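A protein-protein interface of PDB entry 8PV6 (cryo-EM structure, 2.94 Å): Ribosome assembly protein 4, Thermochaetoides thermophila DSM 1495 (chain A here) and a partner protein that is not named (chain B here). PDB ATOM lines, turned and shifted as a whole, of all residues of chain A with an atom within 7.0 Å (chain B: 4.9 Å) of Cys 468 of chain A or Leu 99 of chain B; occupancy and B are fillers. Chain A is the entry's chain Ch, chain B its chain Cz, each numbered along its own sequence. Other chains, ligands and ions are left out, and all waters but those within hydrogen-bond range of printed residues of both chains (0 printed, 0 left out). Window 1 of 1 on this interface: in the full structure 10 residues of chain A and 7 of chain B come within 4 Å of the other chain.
Printed residues of chain B that touch a printed residue of chain A: Arg 95, Tyr 96, Leu 99 and Met 103.
Hydrophobic or aromatic side chains of chain B within 4 Å of the printed part of chain A: Tyr 96, Leu 99 and Met 103.
Printed residues of chain A that touch a printed residue of chain B: Asp 467, Cys 468, Glu 488, Asp 489, Lys 508 and Asp 509.
Among the printed residues, 9 pairs touch across the chains.
Among the printed residues, no Asp or Glu carboxylate lies within 4 Å of a Lys or Arg side-chain nitrogen of the other chain.
CA of Asp 467 of chain A touches SD of Met 103 of chain B, at 3.7 Å.
Cys 468 of chain A touches Leu 99 of chain B (SG to CD2, 3.7 Å).
Glu 488 of chain A touches Tyr 96 of chain B.
Glu 488 of chain A touches Leu 99 of chain B.
OD2 of Asp 489 of chain A touches CE2 of Tyr 96 of chain B (3.2 Å).
OD1 of Asp 489 of chain A touches CD2 of Leu 99 of chain B, 3.3 Å away.
Lys 508 of chain A touches Arg 95 of chain B (CE to NH1, 3.7 Å).
Tyr 96 of chain B touches Asp 509 of chain A (OH to CA, 3.9 Å).
Of chain B, only Leu 99 (3.7 Å) comes within 4 Å of Cys 468 of chain A.
Of chain A, only Cys 468 (3.7 Å), Glu 488 (3.5 Å) and Asp 489 (3.3 Å) come within 4 Å of Leu 99 of chain B.
Of the printed residues of chain B, Asp 489 of chain A touches Tyr 96 and Leu 99.
Of the printed residues of chain B, Glu 488 of chain A touches Tyr 96 and Leu 99.
Of the printed residues of chain B, Lys 508 of chain A touches Arg 95 and Tyr 96.
Of the printed residues of chain A, Arg 95 of chain B touches Lys 508 (3.7 Å).
Of the printed residues of chain B, Asp 509 of chain A touches Tyr 96 (3.9 Å).
The nearest residue of chain B that does not touch Cys 468 of chain A is Met 103 of chain B (4.7 Å).
The nearest residue of chain A that does not touch Leu 99 of chain B is Glu 490 of chain A (4.7 Å).
The nearest printed residue of chain B that does not touch Asp 467 of chain A is Leu 99 of chain B (6.5 Å).
The side-chain hydroxyl (OG) of Ser 465 of chain A lies close to the side-chain carboxylate (OD1) of Asp 467 of chain A, 3.5 Å away.
OD2 of Asp 467 of chain A is in hydrogen-bond range of ND1 of His 445 of chain A (2.8 Å).
O of Glu 490 of chain A lies within hydrogen-bond range of N of Lys 508 of chain A.
The backbone carbonyl oxygen of Asp 489 of chain A lies close to the side-chain sulfur of Cys 468 of chain A, at 3.4 Å.
The guanidinium group (NH2) of Arg 95 of chain B lies close to the side-chain hydroxyl (OH) of Tyr 96 of chain B (3.4 Å).
OD1 of Asp 467 of chain A sits at hydrogen-bond distance from OG1 of Thr 469 of chain A (2.7 Å).
The backbone carbonyl oxygen (O) of Lys 508 of chain A is in hydrogen-bond range of the side-chain hydroxyl (OH) of Tyr 96 of chain B (3.4 Å).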
ATOM      1  N   HIS A 445       9.316  24.707 -18.658  1.00  0.00           N
ATOM      2  CA  HIS A 445       9.508  23.984 -17.413  1.00  0.00           C
ATOM      3  C   HIS A 445      10.415  24.772 -16.469  1.00  0.00           C
ATOM      4  O   HIS A 445      11.163  25.664 -16.873  1.00  0.00           O
ATOM      5  CB  HIS A 445      10.100  22.605 -17.691  1.00  0.00           C
ATOM      6  CG  HIS A 445       9.119  21.631 -18.264  1.00  0.00           C
ATOM      7  ND1 HIS A 445       8.037  21.157 -17.554  1.00  0.00           N
ATOM      8  CD2 HIS A 445       9.054  21.044 -19.482  1.00  0.00           C
ATOM      9  CE1 HIS A 445       7.351  20.319 -18.310  1.00  0.00           C
ATOM     10  NE2 HIS A 445       7.947  20.233 -19.485  1.00  0.00           N
ATOM     11  N   ALA A 447      11.967  22.745 -13.788  1.00  0.00           N
ATOM     12  CA  ALA A 447      12.799  21.679 -13.250  1.00  0.00           C
ATOM     13  C   ALA A 447      13.274  20.842 -14.431  1.00  0.00           C
ATOM     14  O   ALA A 447      12.682  20.950 -15.513  1.00  0.00           O
ATOM     15  CB  ALA A 447      12.014  20.850 -12.231  1.00  0.00           C
ATOM     16  N   GLY A 464       7.623  15.342 -20.280  1.00  0.00           N
ATOM     17  CA  GLY A 464       7.367  15.159 -18.870  1.00  0.00           C
ATOM     18  C   GLY A 464       8.593  15.481 -18.052  1.00  0.00           C
ATOM     19  O   GLY A 464       9.679  14.937 -18.311  1.00  0.00           O
ATOM     20  N   SER A 465       8.437  16.363 -17.066  1.00  0.00           N
ATOM     21  CA  SER A 465       9.596  16.898 -16.369  1.00  0.00           C
ATOM     22  C   SER A 465       9.532  16.606 -14.878  1.00  0.00           C
ATOM     23  O   SER A 465       8.585  16.004 -14.367  1.00  0.00           O
ATOM     24  CB  SER A 465       9.724  18.407 -16.597  1.00  0.00           C
ATOM     25  OG  SER A 465      10.750  18.955 -15.790  1.00  0.00           O
ATOM     26  N   LYS A 466      10.578  17.055 -14.184  1.00  0.00           N
ATOM     27  CA  LYS A 466      10.696  16.937 -12.739  1.00  0.00           C
ATOM     28  C   LYS A 466       9.763  17.893 -12.002  1.00  0.00           C
ATOM     29  O   LYS A 466       9.459  17.664 -10.826  1.00  0.00           O
ATOM     30  CB  LYS A 466      12.164  17.172 -12.350  1.00  0.00           C
ATOM     31  CG  LYS A 466      12.526  17.083 -10.875  1.00  0.00           C
ATOM     32  CD  LYS A 466      13.987  17.441 -10.666  1.00  0.00           C
ATOM     33  CE  LYS A 466      14.384  17.355  -9.205  1.00  0.00           C
ATOM     34  NZ  LYS A 466      15.778  17.830  -8.992  1.00  0.00           N
ATOM     35  N   ASP A 467       9.236  18.913 -12.681  1.00  0.00           N
ATOM     36  CA  ASP A 467       8.362  19.896 -12.053  1.00  0.00           C
ATOM     37  C   ASP A 467       6.915  19.429 -11.929  1.00  0.00           C
ATOM     38  O   ASP A 467       6.022  20.279 -11.835  1.00  0.00           O
ATOM     39  CB  ASP A 467       8.422  21.231 -12.810  1.00  0.00           C
ATOM     40  CG  ASP A 467       7.983  21.124 -14.266  1.00  0.00           C
ATOM     41  OD1 ASP A 467       7.634  20.025 -14.740  1.00  0.00           O
ATOM     42  OD2 ASP A 467       7.989  22.169 -14.949  1.00  0.00           O
ATOM     43  N   CYS A 468       6.677  18.118 -11.967  1.00  0.00           N
ATOM     44  CA  CYS A 468       5.402  17.425 -11.792  1.00  0.00           C
ATOM     45  C   CYS A 468       4.442  17.690 -12.944  1.00  0.00           C
ATOM     46  O   CYS A 468       3.237  17.479 -12.773  1.00  0.00           O
ATOM     47  CB  CYS A 468       4.696  17.789 -10.475  1.00  0.00           C
ATOM     48  SG  CYS A 468       5.785  17.870  -9.041  1.00  0.00           S
ATOM     49  N   THR A 469       4.915  18.151 -14.100  1.00  0.00           N
ATOM     50  CA  THR A 469       4.034  18.514 -15.197  1.00  0.00           C
ATOM     51  C   THR A 469       4.431  17.818 -16.494  1.00  0.00           C
ATOM     52  O   THR A 469       5.608  17.503 -16.743  1.00  0.00           O
ATOM     53  CB  THR A 469       4.013  20.035 -15.442  1.00  0.00           C
ATOM     54  OG1 THR A 469       5.268  20.452 -15.991  1.00  0.00           O
ATOM     55  CG2 THR A 469       3.721  20.813 -14.166  1.00  0.00           C
ATOM     56  N   LEU A 470       3.407  17.594 -17.321  1.00  0.00           N
ATOM     57  CA  LEU A 470       3.567  17.272 -18.728  1.00  0.00           C
ATOM     58  C   LEU A 470       3.249  18.528 -19.525  1.00  0.00           C
ATOM     59  O   LEU A 470       2.392  19.321 -19.127  1.00  0.00           O
ATOM     60  CB  LEU A 470       2.625  16.150 -19.169  1.00  0.00           C
ATOM     61  CG  LEU A 470       2.579  14.805 -18.447  1.00  0.00           C
ATOM     62  CD1 LEU A 470       1.774  13.817 -19.272  1.00  0.00           C
ATOM     63  CD2 LEU A 470       3.950  14.264 -18.155  1.00  0.00           C
ATOM     64  N   LEU A 484      -0.410  19.932 -18.919  1.00  0.00           N
ATOM     65  CA  LEU A 484      -1.035  18.820 -18.211  1.00  0.00           C
ATOM     66  C   LEU A 484      -0.477  18.787 -16.793  1.00  0.00           C
ATOM     67  O   LEU A 484       0.607  18.228 -16.549  1.00  0.00           O
ATOM     68  CB  LEU A 484      -0.793  17.496 -18.931  1.00  0.00           C
ATOM     69  CG  LEU A 484      -1.289  17.412 -20.373  1.00  0.00           C
ATOM     70  CD1 LEU A 484      -0.917  16.074 -20.986  1.00  0.00           C
ATOM     71  CD2 LEU A 484      -2.788  17.634 -20.434  1.00  0.00           C
ATOM     72  N   PRO A 485      -1.159  19.426 -15.846  1.00  0.00           N
ATOM     73  CA  PRO A 485      -0.823  19.230 -14.436  1.00  0.00           C
ATOM     74  C   PRO A 485      -1.664  18.118 -13.835  1.00  0.00           C
ATOM     75  O   PRO A 485      -2.588  17.597 -14.464  1.00  0.00           O
ATOM     76  CB  PRO A 485      -1.161  20.582 -13.806  1.00  0.00           C
ATOM     77  CG  PRO A 485      -2.323  21.056 -14.622  1.00  0.00           C
ATOM     78  CD  PRO A 485      -2.100  20.545 -16.033  1.00  0.00           C
ATOM     79  N   GLY A 486      -1.346  17.769 -12.594  1.00  0.00           N
ATOM     80  CA  GLY A 486      -2.086  16.733 -11.904  1.00  0.00           C
ATOM     81  C   GLY A 486      -1.193  15.811 -11.103  1.00  0.00           C
ATOM     82  O   GLY A 486      -1.611  15.275 -10.073  1.00  0.00           O
ATOM     83  N   HIS A 487       0.038  15.616 -11.569  1.00  0.00           N
ATOM     84  CA  HIS A 487       1.012  14.862 -10.796  1.00  0.00           C
ATOM     85  C   HIS A 487       1.407  15.645  -9.553  1.00  0.00           C
ATOM     86  O   HIS A 487       1.657  16.851  -9.613  1.00  0.00           O
ATOM     87  CB  HIS A 487       2.249  14.561 -11.644  1.00  0.00           C
ATOM     88  CG  HIS A 487       2.086  13.397 -12.569  1.00  0.00           C
ATOM     89  ND1 HIS A 487       2.279  12.094 -12.166  1.00  0.00           N
ATOM     90  CD2 HIS A 487       1.749  13.339 -13.879  1.00  0.00           C
ATOM     91  CE1 HIS A 487       2.068  11.283 -13.188  1.00  0.00           C
ATOM     92  NE2 HIS A 487       1.745  12.014 -14.239  1.00  0.00           N
ATOM     93  N   GLU A 488       1.444  14.955  -8.417  1.00  0.00           N
ATOM     94  CA  GLU A 488       1.842  15.572  -7.162  1.00  0.00           C
ATOM     95  C   GLU A 488       3.328  15.429  -6.879  1.00  0.00           C
ATOM     96  O   GLU A 488       3.801  15.943  -5.860  1.00  0.00           O
ATOM     97  CB  GLU A 488       1.041  14.974  -6.000  1.00  0.00           C
ATOM     98  CG  GLU A 488      -0.463  15.108  -6.155  1.00  0.00           C
ATOM     99  CD  GLU A 488      -1.227  14.174  -5.238  1.00  0.00           C
ATOM    100  OE1 GLU A 488      -0.641  13.168  -4.789  1.00  0.00           O
ATOM    101  OE2 GLU A 488      -2.415  14.447  -4.966  1.00  0.00           O
ATOM    102  N   ASP A 489       4.072  14.755  -7.750  1.00  0.00           N
ATOM    103  CA  ASP A 489       5.496  14.538  -7.552  1.00  0.00           C
ATOM    104  C   ASP A 489       6.150  14.400  -8.923  1.00  0.00           C
ATOM    105  O   ASP A 489       5.522  14.649  -9.957  1.00  0.00           O
ATOM    106  CB  ASP A 489       5.719  13.328  -6.639  1.00  0.00           C
ATOM    107  CG  ASP A 489       6.968  13.460  -5.795  1.00  0.00           C
ATOM    108  OD1 ASP A 489       7.861  14.246  -6.171  1.00  0.00           O
ATOM    109  OD2 ASP A 489       7.054  12.785  -4.748  1.00  0.00           O
ATOM    110  N   GLU A 490       7.425  14.012  -8.926  1.00  0.00           N
ATOM    111  CA  GLU A 490       8.218  13.999 -10.150  1.00  0.00           C
ATOM    112  C   GLU A 490       7.690  12.969 -11.143  1.00  0.00           C
ATOM    113  O   GLU A 490       7.246  11.885 -10.762  1.00  0.00           O
ATOM    114  CB  GLU A 490       9.680  13.701  -9.822  1.00  0.00           C
ATOM    115  CG  GLU A 490      10.252  14.560  -8.708  1.00  0.00           C
ATOM    116  CD  GLU A 490      11.702  14.236  -8.410  1.00  0.00           C
ATOM    117  OE1 GLU A 490      12.359  13.600  -9.261  1.00  0.00           O
ATOM    118  OE2 GLU A 490      12.185  14.616  -7.323  1.00  0.00           O
ATOM    119  N   VAL A 491       7.739  13.322 -12.422  1.00  0.00           N
ATOM    120  CA  VAL A 491       7.282  12.445 -13.493  1.00  0.00           C
ATOM    121  C   VAL A 491       8.480  11.697 -14.058  1.00  0.00           C
ATOM    122  O   VAL A 491       9.449  12.314 -14.517  1.00  0.00           O
ATOM    123  CB  VAL A 491       6.564  13.244 -14.591  1.00  0.00           C
ATOM    124  CG1 VAL A 491       6.152  12.327 -15.721  1.00  0.00           C
ATOM    125  CG2 VAL A 491       5.361  13.966 -14.016  1.00  0.00           C
ATOM    126  N   LYS A 508       6.586   9.574  -9.291  1.00  0.00           N
ATOM    127  CA  LYS A 508       6.744   9.376  -7.858  1.00  0.00           C
ATOM    128  C   LYS A 508       5.427   9.453  -7.097  1.00  0.00           C
ATOM    129  O   LYS A 508       5.400   9.149  -5.900  1.00  0.00           O
ATOM    130  CB  LYS A 508       7.728  10.410  -7.312  1.00  0.00           C
ATOM    131  CG  LYS A 508       8.553   9.965  -6.126  1.00  0.00           C
ATOM    132  CD  LYS A 508       9.601  11.011  -5.799  1.00  0.00           C
ATOM    133  CE  LYS A 508      10.290  10.713  -4.484  1.00  0.00           C
ATOM    134  NZ  LYS A 508      11.211  11.814  -4.088  1.00  0.00           N
ATOM    135  N   ASP A 509       4.337   9.841  -7.759  1.00  0.00           N
ATOM    136  CA  ASP A 509       3.041   9.901  -7.094  1.00  0.00           C
ATOM    137  C   ASP A 509       2.339   8.551  -7.045  1.00  0.00           C
ATOM    138  O   ASP A 509       1.226   8.476  -6.512  1.00  0.00           O
ATOM    139  CB  ASP A 509       2.144  10.932  -7.783  1.00  0.00           C
ATOM    140  CG  ASP A 509       2.058  10.725  -9.283  1.00  0.00           C
ATOM    141  OD1 ASP A 509       2.753   9.830  -9.810  1.00  0.00           O
ATOM    142  OD2 ASP A 509       1.293  11.463  -9.940  1.00  0.00           O
ATOM    143  N   ARG B  95       5.969  16.265   2.615  1.00  0.00           N
ATOM    144  CA  ARG B  95       6.788  16.347   1.410  1.00  0.00           C
ATOM    145  C   ARG B  95       5.974  16.835   0.217  1.00  0.00           C
ATOM    146  O   ARG B  95       6.447  17.667  -0.569  1.00  0.00           O
ATOM    147  CB  ARG B  95       7.419  14.987   1.117  1.00  0.00           C
ATOM    148  CG  ARG B  95       8.178  14.913  -0.196  1.00  0.00           C
ATOM    149  CD  ARG B  95       8.569  13.484  -0.527  1.00  0.00           C
ATOM    150  NE  ARG B  95       7.406  12.618  -0.673  1.00  0.00           N
ATOM    151  CZ  ARG B  95       7.467  11.329  -0.978  1.00  0.00           C
ATOM    152  NH1 ARG B  95       8.625  10.720  -1.176  1.00  0.00           N
ATOM    153  NH2 ARG B  95       6.339  10.634  -1.088  1.00  0.00           N
ATOM    154  N   TYR B  96       4.740  16.342   0.074  1.00  0.00           N
ATOM    155  CA  TYR B  96       3.887  16.784  -1.020  1.00  0.00           C
ATOM    156  C   TYR B  96       3.404  18.217  -0.856  1.00  0.00           C
ATOM    157  O   TYR B  96       2.995  18.828  -1.849  1.00  0.00           O
ATOM    158  CB  TYR B  96       2.685  15.848  -1.172  1.00  0.00           C
ATOM    159  CG  TYR B  96       3.008  14.486  -1.758  1.00  0.00           C
ATOM    160  CD1 TYR B  96       2.026  13.514  -1.876  1.00  0.00           C
ATOM    161  CD2 TYR B  96       4.287  14.181  -2.210  1.00  0.00           C
ATOM    162  CE1 TYR B  96       2.310  12.274  -2.414  1.00  0.00           C
ATOM    163  CE2 TYR B  96       4.579  12.945  -2.746  1.00  0.00           C
ATOM    164  CZ  TYR B  96       3.588  11.996  -2.847  1.00  0.00           C
ATOM    165  OH  TYR B  96       3.876  10.763  -3.384  1.00  0.00           O
ATOM    166  N   GLU B  97       3.427  18.763   0.360  1.00  0.00           N
ATOM    167  CA  GLU B  97       3.174  20.192   0.511  1.00  0.00           C
ATOM    168  C   GLU B  97       4.405  21.030   0.160  1.00  0.00           C
ATOM    169  O   GLU B  97       4.297  22.034  -0.562  1.00  0.00           O
ATOM    170  CB  GLU B  97       2.708  20.489   1.941  1.00  0.00           C
ATOM    171  CG  GLU B  97       2.978  21.904   2.421  1.00  0.00           C
ATOM    172  CD  GLU B  97       2.779  22.062   3.915  1.00  0.00           C
ATOM    173  OE1 GLU B  97       2.127  21.188   4.524  1.00  0.00           O
ATOM    174  OE2 GLU B  97       3.275  23.058   4.481  1.00  0.00           O
ATOM    175  N   GLN B  98       5.579  20.619   0.654  1.00  0.00           N
ATOM    176  CA  GLN B  98       6.798  21.396   0.437  1.00  0.00           C
ATOM    177  C   GLN B  98       7.195  21.433  -1.034  1.00  0.00           C
ATOM    178  O   GLN B  98       7.673  22.463  -1.526  1.00  0.00           O
ATOM    179  CB  GLN B  98       7.943  20.835   1.278  1.00  0.00           C
ATOM    180  CG  GLN B  98       7.755  20.995   2.775  1.00  0.00           C
ATOM    181  CD  GLN B  98       8.904  20.406   3.567  1.00  0.00           C
ATOM    182  OE1 GLN B  98       9.822  19.814   3.002  1.00  0.00           O
ATOM    183  NE2 GLN B  98       8.858  20.566   4.884  1.00  0.00           N
ATOM    184  N   LEU B  99       7.015  20.318  -1.750  1.00  0.00           N
ATOM    185  CA  LEU B  99       7.358  20.290  -3.169  1.00  0.00           C
ATOM    186  C   LEU B  99       6.479  21.239  -3.978  1.00  0.00           C
ATOM    187  O   LEU B  99       6.971  21.949  -4.866  1.00  0.00           O
ATOM    188  CB  LEU B  99       7.235  18.866  -3.702  1.00  0.00           C
ATOM    189  CG  LEU B  99       7.386  18.712  -5.210  1.00  0.00           C
ATOM    190  CD1 LEU B  99       8.815  18.989  -5.640  1.00  0.00           C
ATOM    191  CD2 LEU B  99       6.958  17.329  -5.615  1.00  0.00           C
ATOM    192  N   ALA B 100       5.178  21.265  -3.679  1.00  0.00           N
ATOM    193  CA  ALA B 100       4.273  22.183  -4.365  1.00  0.00           C
ATOM    194  C   ALA B 100       4.621  23.631  -4.054  1.00  0.00           C
ATOM    195  O   ALA B 100       4.559  24.495  -4.939  1.00  0.00           O
ATOM    196  CB  ALA B 100       2.826  21.883  -3.976  1.00  0.00           C
ATOM    197  N   ALA B 101       5.000  23.910  -2.802  1.00  0.00           N
ATOM    198  CA  ALA B 101       5.437  25.258  -2.442  1.00  0.00           C
ATOM    199  C   ALA B 101       6.682  25.665  -3.225  1.00  0.00           C
ATOM    200  O   ALA B 101       6.775  26.793  -3.727  1.00  0.00           O
ATOM    201  CB  ALA B 101       5.696  25.337  -0.938  1.00  0.00           C
ATOM    202  N   LYS B 102       7.642  24.743  -3.355  1.00  0.00           N
ATOM    203  CA  LYS B 102       8.870  25.033  -4.092  1.00  0.00           C
ATOM    204  C   LYS B 102       8.588  25.290  -5.569  1.00  0.00           C
ATOM    205  O   LYS B 102       9.160  26.207  -6.171  1.00  0.00           O
ATOM    206  CB  LYS B 102       9.859  23.881  -3.928  1.00  0.00           C
ATOM    207  CG  LYS B 102      11.194  24.113  -4.611  1.00  0.00           C
ATOM    208  CD  LYS B 102      12.097  22.900  -4.479  1.00  0.00           C
ATOM    209  CE  LYS B 102      12.601  22.747  -3.057  1.00  0.00           C
ATOM    210  NZ  LYS B 102      13.521  23.854  -2.677  1.00  0.00           N
ATOM    211  N   MET B 103       7.704  24.489  -6.171  1.00  0.00           N
ATOM    212  CA  MET B 103       7.382  24.682  -7.584  1.00  0.00           C
ATOM    213  C   MET B 103       6.636  25.991  -7.818  1.00  0.00           C
ATOM    214  O   MET B 103       6.872  26.677  -8.822  1.00  0.00           O
ATOM    215  CB  MET B 103       6.574  23.498  -8.109  1.00  0.00           C
ATOM    216  CG  MET B 103       7.319  22.169  -8.129  1.00  0.00           C
ATOM    217  SD  MET B 103       8.784  22.142  -9.184  1.00  0.00           S
ATOM    218  CE  MET B 103      10.111  22.295  -7.990  1.00  0.00           C
